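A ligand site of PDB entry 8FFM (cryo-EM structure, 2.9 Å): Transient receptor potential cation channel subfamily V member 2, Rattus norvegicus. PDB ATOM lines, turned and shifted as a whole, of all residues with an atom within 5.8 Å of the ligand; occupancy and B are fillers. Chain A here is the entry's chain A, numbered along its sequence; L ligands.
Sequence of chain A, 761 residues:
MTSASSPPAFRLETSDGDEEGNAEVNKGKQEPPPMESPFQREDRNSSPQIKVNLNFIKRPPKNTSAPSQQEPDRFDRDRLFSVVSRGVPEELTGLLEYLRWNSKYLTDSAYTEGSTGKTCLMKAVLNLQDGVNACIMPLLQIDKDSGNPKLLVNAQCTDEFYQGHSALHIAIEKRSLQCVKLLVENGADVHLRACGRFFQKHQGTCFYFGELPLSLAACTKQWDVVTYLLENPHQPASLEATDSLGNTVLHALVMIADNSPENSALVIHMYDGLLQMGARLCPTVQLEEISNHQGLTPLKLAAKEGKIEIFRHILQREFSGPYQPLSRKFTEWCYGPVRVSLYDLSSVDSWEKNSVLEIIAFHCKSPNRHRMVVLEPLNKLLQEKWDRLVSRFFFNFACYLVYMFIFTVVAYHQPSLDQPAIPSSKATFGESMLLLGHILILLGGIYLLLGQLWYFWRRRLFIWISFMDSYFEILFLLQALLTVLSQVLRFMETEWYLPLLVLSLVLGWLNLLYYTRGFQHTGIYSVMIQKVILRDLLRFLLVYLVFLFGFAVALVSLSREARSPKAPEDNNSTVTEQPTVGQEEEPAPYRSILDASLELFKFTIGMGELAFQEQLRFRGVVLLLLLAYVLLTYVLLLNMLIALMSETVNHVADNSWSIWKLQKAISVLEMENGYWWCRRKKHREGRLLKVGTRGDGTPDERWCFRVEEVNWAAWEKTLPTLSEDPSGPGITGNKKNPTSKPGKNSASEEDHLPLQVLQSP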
ATOM      1  N   PHE A 395      -2.707  14.957  -7.321  1.00  0.00           N
ATOM      2  CA  PHE A 395      -2.952  14.249  -6.077  1.00  0.00           C
ATOM      3  C   PHE A 395      -4.241  14.703  -5.403  1.00  0.00           C
ATOM      4  O   PHE A 395      -5.082  13.883  -5.068  1.00  0.00           O
ATOM      5  CB  PHE A 395      -1.756  14.412  -5.174  1.00  0.00           C
ATOM      6  CG  PHE A 395      -1.936  13.760  -3.832  1.00  0.00           C
ATOM      7  CD1 PHE A 395      -1.765  12.377  -3.686  1.00  0.00           C
ATOM      8  CD2 PHE A 395      -2.256  14.546  -2.708  1.00  0.00           C
ATOM      9  CE1 PHE A 395      -1.891  11.778  -2.434  1.00  0.00           C
ATOM     10  CE2 PHE A 395      -2.380  13.949  -1.447  1.00  0.00           C
ATOM     11  CZ  PHE A 395      -2.212  12.565  -1.310  1.00  0.00           C
ATOM     12  N   ASN A 396      -4.488  15.998  -5.267  1.00  0.00           N
ATOM     13  CA  ASN A 396      -5.756  16.499  -4.734  1.00  0.00           C
ATOM     14  C   ASN A 396      -6.954  16.007  -5.531  1.00  0.00           C
ATOM     15  O   ASN A 396      -7.946  15.592  -4.948  1.00  0.00           O
ATOM     16  CB  ASN A 396      -5.707  18.032  -4.731  1.00  0.00           C
ATOM     17  CG  ASN A 396      -4.891  18.613  -3.619  1.00  0.00           C
ATOM     18  OD1 ASN A 396      -4.399  17.937  -2.735  1.00  0.00           O
ATOM     19  ND2 ASN A 396      -4.791  19.909  -3.582  1.00  0.00           N
ATOM     20  N   PHE A 397      -6.862  16.005  -6.855  1.00  0.00           N
ATOM     21  CA  PHE A 397      -7.909  15.472  -7.711  1.00  0.00           C
ATOM     22  C   PHE A 397      -8.119  13.974  -7.533  1.00  0.00           C
ATOM     23  O   PHE A 397      -9.249  13.526  -7.495  1.00  0.00           O
ATOM     24  CB  PHE A 397      -7.517  15.761  -9.145  1.00  0.00           C
ATOM     25  CG  PHE A 397      -8.467  15.216 -10.173  1.00  0.00           C
ATOM     26  CD1 PHE A 397      -9.844  15.423 -10.056  1.00  0.00           C
ATOM     27  CD2 PHE A 397      -7.958  14.567 -11.306  1.00  0.00           C
ATOM     28  CE1 PHE A 397     -10.712  15.009 -11.075  1.00  0.00           C
ATOM     29  CE2 PHE A 397      -8.823  14.140 -12.314  1.00  0.00           C
ATOM     30  CZ  PHE A 397     -10.197  14.366 -12.211  1.00  0.00           C
ATOM     31  N   ALA A 398      -7.051  13.197  -7.373  1.00  0.00           N
ATOM     32  CA  ALA A 398      -7.147  11.794  -7.066  1.00  0.00           C
ATOM     33  C   ALA A 398      -7.859  11.573  -5.741  1.00  0.00           C
ATOM     34  O   ALA A 398      -8.773  10.754  -5.679  1.00  0.00           O
ATOM     35  CB  ALA A 398      -5.747  11.191  -7.045  1.00  0.00           C
ATOM     36  N   CYS A 399      -7.532  12.303  -4.689  1.00  0.00           N
ATOM     37  CA  CYS A 399      -8.235  12.132  -3.427  1.00  0.00           C
ATOM     38  C   CYS A 399      -9.701  12.496  -3.533  1.00  0.00           C
ATOM     39  O   CYS A 399     -10.534  11.784  -3.011  1.00  0.00           O
ATOM     40  CB  CYS A 399      -7.577  12.958  -2.332  1.00  0.00           C
ATOM     41  SG  CYS A 399      -5.875  12.428  -2.160  1.00  0.00           S
ATOM     42  N   TYR A 400     -10.033  13.566  -4.245  1.00  0.00           N
ATOM     43  CA  TYR A 400     -11.418  13.917  -4.464  1.00  0.00           C
ATOM     44  C   TYR A 400     -12.154  12.862  -5.267  1.00  0.00           C
ATOM     45  O   TYR A 400     -13.276  12.524  -4.915  1.00  0.00           O
ATOM     46  CB  TYR A 400     -11.504  15.285  -5.097  1.00  0.00           C
ATOM     47  CG  TYR A 400     -12.916  15.805  -5.104  1.00  0.00           C
ATOM     48  CD1 TYR A 400     -13.472  16.288  -3.923  1.00  0.00           C
ATOM     49  CD2 TYR A 400     -13.667  15.771  -6.287  1.00  0.00           C
ATOM     50  CE1 TYR A 400     -14.802  16.726  -3.905  1.00  0.00           C
ATOM     51  CE2 TYR A 400     -14.984  16.237  -6.277  1.00  0.00           C
ATOM     52  CZ  TYR A 400     -15.553  16.707  -5.090  1.00  0.00           C
ATOM     53  OH  TYR A 400     -16.827  17.130  -5.079  1.00  0.00           O
ATOM     54  N   VAL A 402     -11.423   9.552  -5.277  1.00  0.00           N
ATOM     55  CA  VAL A 402     -11.604   8.428  -4.356  1.00  0.00           C
ATOM     56  C   VAL A 402     -12.740   8.704  -3.404  1.00  0.00           C
ATOM     57  O   VAL A 402     -13.634   7.875  -3.262  1.00  0.00           O
ATOM     58  CB  VAL A 402     -10.307   8.110  -3.620  1.00  0.00           C
ATOM     59  CG1 VAL A 402     -10.521   7.152  -2.441  1.00  0.00           C
ATOM     60  CG2 VAL A 402      -9.331   7.451  -4.595  1.00  0.00           C
ATOM     61  N   TYR A 403     -12.786   9.882  -2.789  1.00  0.00           N
ATOM     62  CA  TYR A 403     -13.883  10.255  -1.927  1.00  0.00           C
ATOM     63  C   TYR A 403     -15.211  10.187  -2.678  1.00  0.00           C
ATOM     64  O   TYR A 403     -16.150   9.591  -2.187  1.00  0.00           O
ATOM     65  CB  TYR A 403     -13.622  11.632  -1.349  1.00  0.00           C
ATOM     66  CG  TYR A 403     -14.831  12.310  -0.721  1.00  0.00           C
ATOM     67  CD1 TYR A 403     -15.143  12.098   0.633  1.00  0.00           C
ATOM     68  CD2 TYR A 403     -15.557  13.240  -1.480  1.00  0.00           C
ATOM     69  CE1 TYR A 403     -16.170  12.859   1.219  1.00  0.00           C
ATOM     70  CE2 TYR A 403     -16.576  13.993  -0.895  1.00  0.00           C
ATOM     71  CZ  TYR A 403     -16.870  13.812   0.469  1.00  0.00           C
ATOM     72  OH  TYR A 403     -17.826  14.567   1.063  1.00  0.00           O
ATOM     73  N   GLY A 444     -14.240  12.596   5.398  1.00  0.00           N
ATOM     74  CA  GLY A 444     -13.986  13.373   4.196  1.00  0.00           C
ATOM     75  C   GLY A 444     -14.819  14.653   4.157  1.00  0.00           C
ATOM     76  O   GLY A 444     -14.295  15.702   3.819  1.00  0.00           O
ATOM     77  N   TYR A 447     -13.251  17.042   6.816  1.00  0.00           N
ATOM     78  CA  TYR A 447     -12.007  17.522   6.264  1.00  0.00           C
ATOM     79  C   TYR A 447     -12.238  18.612   5.236  1.00  0.00           C
ATOM     80  O   TYR A 447     -11.655  19.685   5.322  1.00  0.00           O
ATOM     81  CB  TYR A 447     -11.287  16.321   5.671  1.00  0.00           C
ATOM     82  CG  TYR A 447      -9.991  16.680   4.999  1.00  0.00           C
ATOM     83  CD1 TYR A 447      -8.816  16.688   5.747  1.00  0.00           C
ATOM     84  CD2 TYR A 447      -9.977  17.014   3.638  1.00  0.00           C
ATOM     85  CE1 TYR A 447      -7.610  17.060   5.137  1.00  0.00           C
ATOM     86  CE2 TYR A 447      -8.765  17.378   3.026  1.00  0.00           C
ATOM     87  CZ  TYR A 447      -7.583  17.394   3.772  1.00  0.00           C
ATOM     88  OH  TYR A 447      -6.414  17.740   3.189  1.00  0.00           O
ATOM     89  N   LEU A 448     -13.137  18.405   4.287  1.00  0.00           N
ATOM     90  CA  LEU A 448     -13.481  19.421   3.308  1.00  0.00           C
ATOM     91  C   LEU A 448     -14.120  20.630   3.957  1.00  0.00           C
ATOM     92  O   LEU A 448     -13.810  21.750   3.578  1.00  0.00           O
ATOM     93  CB  LEU A 448     -14.380  18.822   2.237  1.00  0.00           C
ATOM     94  CG  LEU A 448     -13.679  17.805   1.340  1.00  0.00           C
ATOM     95  CD1 LEU A 448     -14.696  17.080   0.476  1.00  0.00           C
ATOM     96  CD2 LEU A 448     -12.674  18.470   0.411  1.00  0.00           C
ATOM     97  N   GLN A 452     -12.541  24.409   3.617  1.00  0.00           N
ATOM     98  CA  GLN A 452     -13.281  25.544   3.083  1.00  0.00           C
ATOM     99  C   GLN A 452     -13.500  26.655   4.109  1.00  0.00           C
ATOM    100  O   GLN A 452     -13.457  27.824   3.754  1.00  0.00           O
ATOM    101  CB  GLN A 452     -14.616  25.085   2.512  1.00  0.00           C
ATOM    102  CG  GLN A 452     -14.470  24.151   1.308  1.00  0.00           C
ATOM    103  CD  GLN A 452     -13.493  24.697   0.286  1.00  0.00           C
ATOM    104  OE1 GLN A 452     -12.385  24.222   0.170  1.00  0.00           O
ATOM    105  NE2 GLN A 452     -13.844  25.746  -0.417  1.00  0.00           N
ATOM    106  N   PHE A 472     -16.835  27.880  -7.139  1.00  0.00           N
ATOM    107  CA  PHE A 472     -16.448  26.547  -6.722  1.00  0.00           C
ATOM    108  C   PHE A 472     -16.070  26.475  -5.245  1.00  0.00           C
ATOM    109  O   PHE A 472     -16.346  25.463  -4.625  1.00  0.00           O
ATOM    110  CB  PHE A 472     -15.335  25.996  -7.589  1.00  0.00           C
ATOM    111  CG  PHE A 472     -15.839  25.364  -8.859  1.00  0.00           C
ATOM    112  CD1 PHE A 472     -16.605  24.186  -8.793  1.00  0.00           C
ATOM    113  CD2 PHE A 472     -15.529  25.925 -10.096  1.00  0.00           C
ATOM    114  CE1 PHE A 472     -17.060  23.595  -9.967  1.00  0.00           C
ATOM    115  CE2 PHE A 472     -15.971  25.320 -11.273  1.00  0.00           C
ATOM    116  CZ  PHE A 472     -16.750  24.155 -11.204  1.00  0.00           C
ATOM    117  N   GLU A 473     -15.507  27.491  -4.632  1.00  0.00           N
ATOM    118  CA  GLU A 473     -15.192  27.440  -3.210  1.00  0.00           C
ATOM    119  C   GLU A 473     -16.444  27.446  -2.353  1.00  0.00           C
ATOM    120  O   GLU A 473     -16.495  26.771  -1.332  1.00  0.00           O
ATOM    121  CB  GLU A 473     -14.243  28.575  -2.833  1.00  0.00           C
ATOM    122  CG  GLU A 473     -12.907  28.489  -3.592  1.00  0.00           C
ATOM    123  CD  GLU A 473     -12.111  27.225  -3.253  1.00  0.00           C
ATOM    124  OE1 GLU A 473     -11.945  26.915  -2.066  1.00  0.00           O
ATOM    125  OE2 GLU A 473     -11.698  26.499  -4.182  1.00  0.00           O
ATOM    126  N   PHE A 476     -17.960  23.786  -2.980  1.00  0.00           N
ATOM    127  CA  PHE A 476     -17.243  22.815  -2.138  1.00  0.00           C
ATOM    128  C   PHE A 476     -17.635  22.951  -0.672  1.00  0.00           C
ATOM    129  O   PHE A 476     -17.777  21.932  -0.013  1.00  0.00           O
ATOM    130  CB  PHE A 476     -15.735  22.952  -2.313  1.00  0.00           C
ATOM    131  CG  PHE A 476     -15.169  22.050  -3.370  1.00  0.00           C
ATOM    132  CD1 PHE A 476     -15.357  22.331  -4.727  1.00  0.00           C
ATOM    133  CD2 PHE A 476     -14.455  20.909  -2.996  1.00  0.00           C
ATOM    134  CE1 PHE A 476     -14.793  21.509  -5.708  1.00  0.00           C
ATOM    135  CE2 PHE A 476     -13.907  20.071  -3.981  1.00  0.00           C
ATOM    136  CZ  PHE A 476     -14.079  20.368  -5.335  1.00  0.00           C
ATOM    137  N   TYR A 514     -14.405  21.479 -11.361  1.00  0.00           N
ATOM    138  CA  TYR A 514     -13.326  22.366 -10.935  1.00  0.00           C
ATOM    139  C   TYR A 514     -11.975  21.967 -11.520  1.00  0.00           C
ATOM    140  O   TYR A 514     -11.233  22.799 -12.036  1.00  0.00           O
ATOM    141  CB  TYR A 514     -13.275  22.380  -9.416  1.00  0.00           C
ATOM    142  CG  TYR A 514     -12.074  23.092  -8.862  1.00  0.00           C
ATOM    143  CD1 TYR A 514     -12.096  24.485  -8.710  1.00  0.00           C
ATOM    144  CD2 TYR A 514     -10.920  22.378  -8.548  1.00  0.00           C
ATOM    145  CE1 TYR A 514     -10.950  25.163  -8.249  1.00  0.00           C
ATOM    146  CE2 TYR A 514      -9.764  23.045  -8.121  1.00  0.00           C
ATOM    147  CZ  TYR A 514      -9.773  24.438  -7.974  1.00  0.00           C
ATOM    148  OH  TYR A 514      -8.663  25.080  -7.570  1.00  0.00           O
ATOM    149  N   TYR A 515     -11.675  20.671 -11.547  1.00  0.00           N
ATOM    150  CA  TYR A 515     -10.393  20.162 -11.977  1.00  0.00           C
ATOM    151  C   TYR A 515     -10.178  20.226 -13.470  1.00  0.00           C
ATOM    152  O   TYR A 515      -9.061  20.053 -13.927  1.00  0.00           O
ATOM    153  CB  TYR A 515     -10.206  18.755 -11.438  1.00  0.00           C
ATOM    154  CG  TYR A 515     -10.208  18.751  -9.942  1.00  0.00           C
ATOM    155  CD1 TYR A 515      -9.020  19.003  -9.239  1.00  0.00           C
ATOM    156  CD2 TYR A 515     -11.396  18.532  -9.250  1.00  0.00           C
ATOM    157  CE1 TYR A 515      -9.019  19.009  -7.841  1.00  0.00           C
ATOM    158  CE2 TYR A 515     -11.395  18.509  -7.849  1.00  0.00           C
ATOM    159  CZ  TYR A 515     -10.204  18.749  -7.135  1.00  0.00           C
ATOM    160  OH  TYR A 515     -10.229  18.712  -5.787  1.00  0.00           O
ATOM    161  N   TYR A 675      -1.916  22.723   3.068  1.00  0.00           N
ATOM    162  CA  TYR A 675      -3.223  22.421   3.620  1.00  0.00           C
ATOM    163  C   TYR A 675      -3.482  23.065   4.975  1.00  0.00           C
ATOM    164  O   TYR A 675      -2.557  23.335   5.736  1.00  0.00           O
ATOM    165  CB  TYR A 675      -3.336  20.906   3.712  1.00  0.00           C
ATOM    166  CG  TYR A 675      -3.026  20.185   2.424  1.00  0.00           C
ATOM    167  CD1 TYR A 675      -3.877  20.345   1.326  1.00  0.00           C
ATOM    168  CD2 TYR A 675      -1.926  19.322   2.337  1.00  0.00           C
ATOM    169  CE1 TYR A 675      -3.624  19.649   0.129  1.00  0.00           C
ATOM    170  CE2 TYR A 675      -1.663  18.619   1.148  1.00  0.00           C
ATOM    171  CZ  TYR A 675      -2.517  18.779   0.041  1.00  0.00           C
ATOM    172  OH  TYR A 675      -2.287  18.089  -1.095  1.00  0.00           O
ATOM    173  N   TRP A 676      -4.748  23.198   5.351  1.00  0.00           N
ATOM    174  CA  TRP A 676      -5.142  23.741   6.649  1.00  0.00           C
ATOM    175  C   TRP A 676      -4.500  23.019   7.838  1.00  0.00           C
ATOM    176  O   TRP A 676      -4.245  23.631   8.866  1.00  0.00           O
ATOM    177  CB  TRP A 676      -6.672  23.709   6.754  1.00  0.00           C
ATOM    178  CG  TRP A 676      -7.298  22.351   6.847  1.00  0.00           C
ATOM    179  CD1 TRP A 676      -7.755  21.606   5.810  1.00  0.00           C
ATOM    180  CD2 TRP A 676      -7.528  21.529   8.035  1.00  0.00           C
ATOM    181  NE1 TRP A 676      -8.254  20.415   6.275  1.00  0.00           N
ATOM    182  CE2 TRP A 676      -8.118  20.304   7.640  1.00  0.00           C
ATOM    183  CE3 TRP A 676      -7.290  21.721   9.411  1.00  0.00           C
ATOM    184  CZ2 TRP A 676      -8.441  19.299   8.553  1.00  0.00           C
ATOM    185  CZ3 TRP A 676      -7.620  20.718  10.348  1.00  0.00           C
ATOM    186  CH2 TRP A 676      -8.184  19.511   9.920  1.00  0.00           C
ATOM    187  N   TRP A 677      -4.213  21.732   7.707  1.00  0.00           N
ATOM    188  CA  TRP A 677      -3.606  20.897   8.741  1.00  0.00           C
ATOM    189  C   TRP A 677      -2.084  20.795   8.645  1.00  0.00           C
ATOM    190  O   TRP A 677      -1.472  20.129   9.485  1.00  0.00           O
ATOM    191  CB  TRP A 677      -4.258  19.524   8.653  1.00  0.00           C
ATOM    192  CG  TRP A 677      -4.058  18.827   7.347  1.00  0.00           C
ATOM    193  CD1 TRP A 677      -4.861  18.942   6.280  1.00  0.00           C
ATOM    194  CD2 TRP A 677      -2.977  17.955   6.948  1.00  0.00           C
ATOM    195  NE1 TRP A 677      -4.344  18.198   5.242  1.00  0.00           N
ATOM    196  CE2 TRP A 677      -3.162  17.602   5.585  1.00  0.00           C
ATOM    197  CE3 TRP A 677      -1.846  17.415   7.590  1.00  0.00           C
ATOM    198  CZ2 TRP A 677      -2.262  16.803   4.877  1.00  0.00           C
ATOM    199  CZ3 TRP A 677      -0.942  16.590   6.895  1.00  0.00           C
ATOM    200  CH2 TRP A 677      -1.145  16.302   5.540  1.00  0.00           C
HETATM  201  O1  LIG L   1      -8.821  20.442  -4.377  1.00  0.00           O
HETATM  202  O2  LIG L   1      -7.576  21.619  -2.636  1.00  0.00           O
HETATM  203  P1  LIG L   1      -8.780  20.843  -2.958  1.00  0.00           P
HETATM  204  O3  LIG L   1      -8.946  19.588  -2.004  1.00  0.00           O
HETATM  205  C1  LIG L   1      -8.158  18.432  -2.232  1.00  0.00           C
HETATM  206  C2  LIG L   1      -8.501  17.413  -1.139  1.00  0.00           C
HETATM  207  C3  LIG L   1      -9.731  16.571  -1.464  1.00  0.00           C
HETATM  208  O4  LIG L   1     -10.001  15.797  -0.289  1.00  0.00           O
HETATM  209  C4  LIG L   1     -11.116  15.040  -0.228  1.00  0.00           C
HETATM  210  O5  LIG L   1     -11.944  14.970  -1.113  1.00  0.00           O
HETATM  211  C5  LIG L   1     -11.101  14.125   0.982  1.00  0.00           C
HETATM  212  C6  LIG L   1     -10.047  13.020   0.783  1.00  0.00           C
HETATM  213  C7  LIG L   1      -9.961  12.029   1.945  1.00  0.00           C
HETATM  214  C8  LIG L   1      -8.890  10.938   1.685  1.00  0.00           C
HETATM  215  C9  LIG L   1      -9.375   9.832   0.724  1.00  0.00           C
HETATM  216  C10 LIG L   1      -8.291   8.778   0.412  1.00  0.00           C
HETATM  217  C11 LIG L   1      -7.253   9.273  -0.625  1.00  0.00           C
HETATM  218  C12 LIG L   1      -6.328   8.146  -1.107  1.00  0.00           C
HETATM  219  C13 LIG L   1      -5.413   8.605  -2.256  1.00  0.00           C
HETATM  220  O6  LIG L   1      -7.381  16.526  -0.951  1.00  0.00           O
HETATM  221  C14 LIG L   1      -6.412  16.916  -0.093  1.00  0.00           C
HETATM  222  O7  LIG L   1      -6.449  17.960   0.536  1.00  0.00           O
HETATM  223  C15 LIG L   1      -5.303  15.888   0.052  1.00  0.00           C
HETATM  224  C16 LIG L   1      -5.782  14.512   0.566  1.00  0.00           C
HETATM  225  C17 LIG L   1      -5.856  14.362   2.106  1.00  0.00           C
HETATM  226  C18 LIG L   1      -4.451  14.360   2.743  1.00  0.00           C
HETATM  227  C19 LIG L   1      -4.392  13.622   4.107  1.00  0.00           C
HETATM  228  C20 LIG L   1      -5.192  14.349   5.215  1.00  0.00           C
HETATM  229  C21 LIG L   1      -4.653  14.024   6.636  1.00  0.00           C
HETATM  230  C22 LIG L   1      -5.312  14.919   7.705  1.00  0.00           C
HETATM  231  C23 LIG L   1      -4.682  14.755   9.095  1.00  0.00           C
HETATM  232  O8  LIG L   1     -10.109  21.592  -2.488  1.00  0.00           O
HETATM  233  C24 LIG L   1     -10.479  22.906  -2.941  1.00  0.00           C
HETATM  234  C25 LIG L   1     -10.609  22.918  -4.476  1.00  0.00           C
HETATM  235  N1  LIG L   1     -11.630  23.913  -5.011  1.00  0.00           N
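OE2 of Glu 473 lies within salt-bridge range of N1 of the ligand. OH of Tyr 515 lies within hydrogen-bond range of O1 of the ligand. The side-chain hydroxyl (OH) of Tyr 447 is in hydrogen-bond range of an oxygen (O7) of the ligand, 2.7 Å away. ND2 of Asn 396 sits at hydrogen-bond distance from O2 of the ligand (3.4 Å).
OH of Tyr 447 lies within hydrogen-bond range of NE1 of Trp 677 (3.0 Å). OH of Tyr 675 is in hydrogen-bond range of OD1 of Asn 396 (2.7 Å). The side-chain carboxylate of Glu 473 sits at hydrogen-bond distance from the side-chain amide nitrogen of Gln 452. SG of Cys 399 sits at hydrogen-bond distance from O of Phe 395 (3.3 Å).
Phe 395 touches the ligand (CE2 to C15, 3.8 Å). Cys 399 touches the ligand (SG to C16, 3.4 Å). Tyr 400 touches the ligand. Val 402 touches the ligand. Tyr 403 touches the ligand (CB to O5, 3.7 Å). Leu 448 touches the ligand (CD1 to O5, 3.8 Å). Gln 452 touches the ligand (OE1 to C24, 3.9 Å). Tyr 514 touches the ligand (CZ to N1, 3.5 Å). CE1 of Tyr 675 touches O7 of the ligand, 3.3 Å away. Trp 677 touches the ligand. Hydrophobic or aromatic side chains within 4 Å of the ligand: Phe 395, Tyr 400, Val 402, Tyr 403, Tyr 447, Leu 448, Tyr 514, Tyr 515, Tyr 675 and Trp 677. Within 4 Å of the ligand: Phe 395, Asn 396, Cys 399, Tyr 400, Val 402, Tyr 403, Tyr 447, Leu 448, Gln 452, Glu 473, Tyr 514, Tyr 515, Tyr 675 and Trp 677. Along chain A the residues within 4 Å of the ligand span positions 395 to 677. The nearest printed residue that does not touch the ligand is Phe 476 (4.03 Å).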
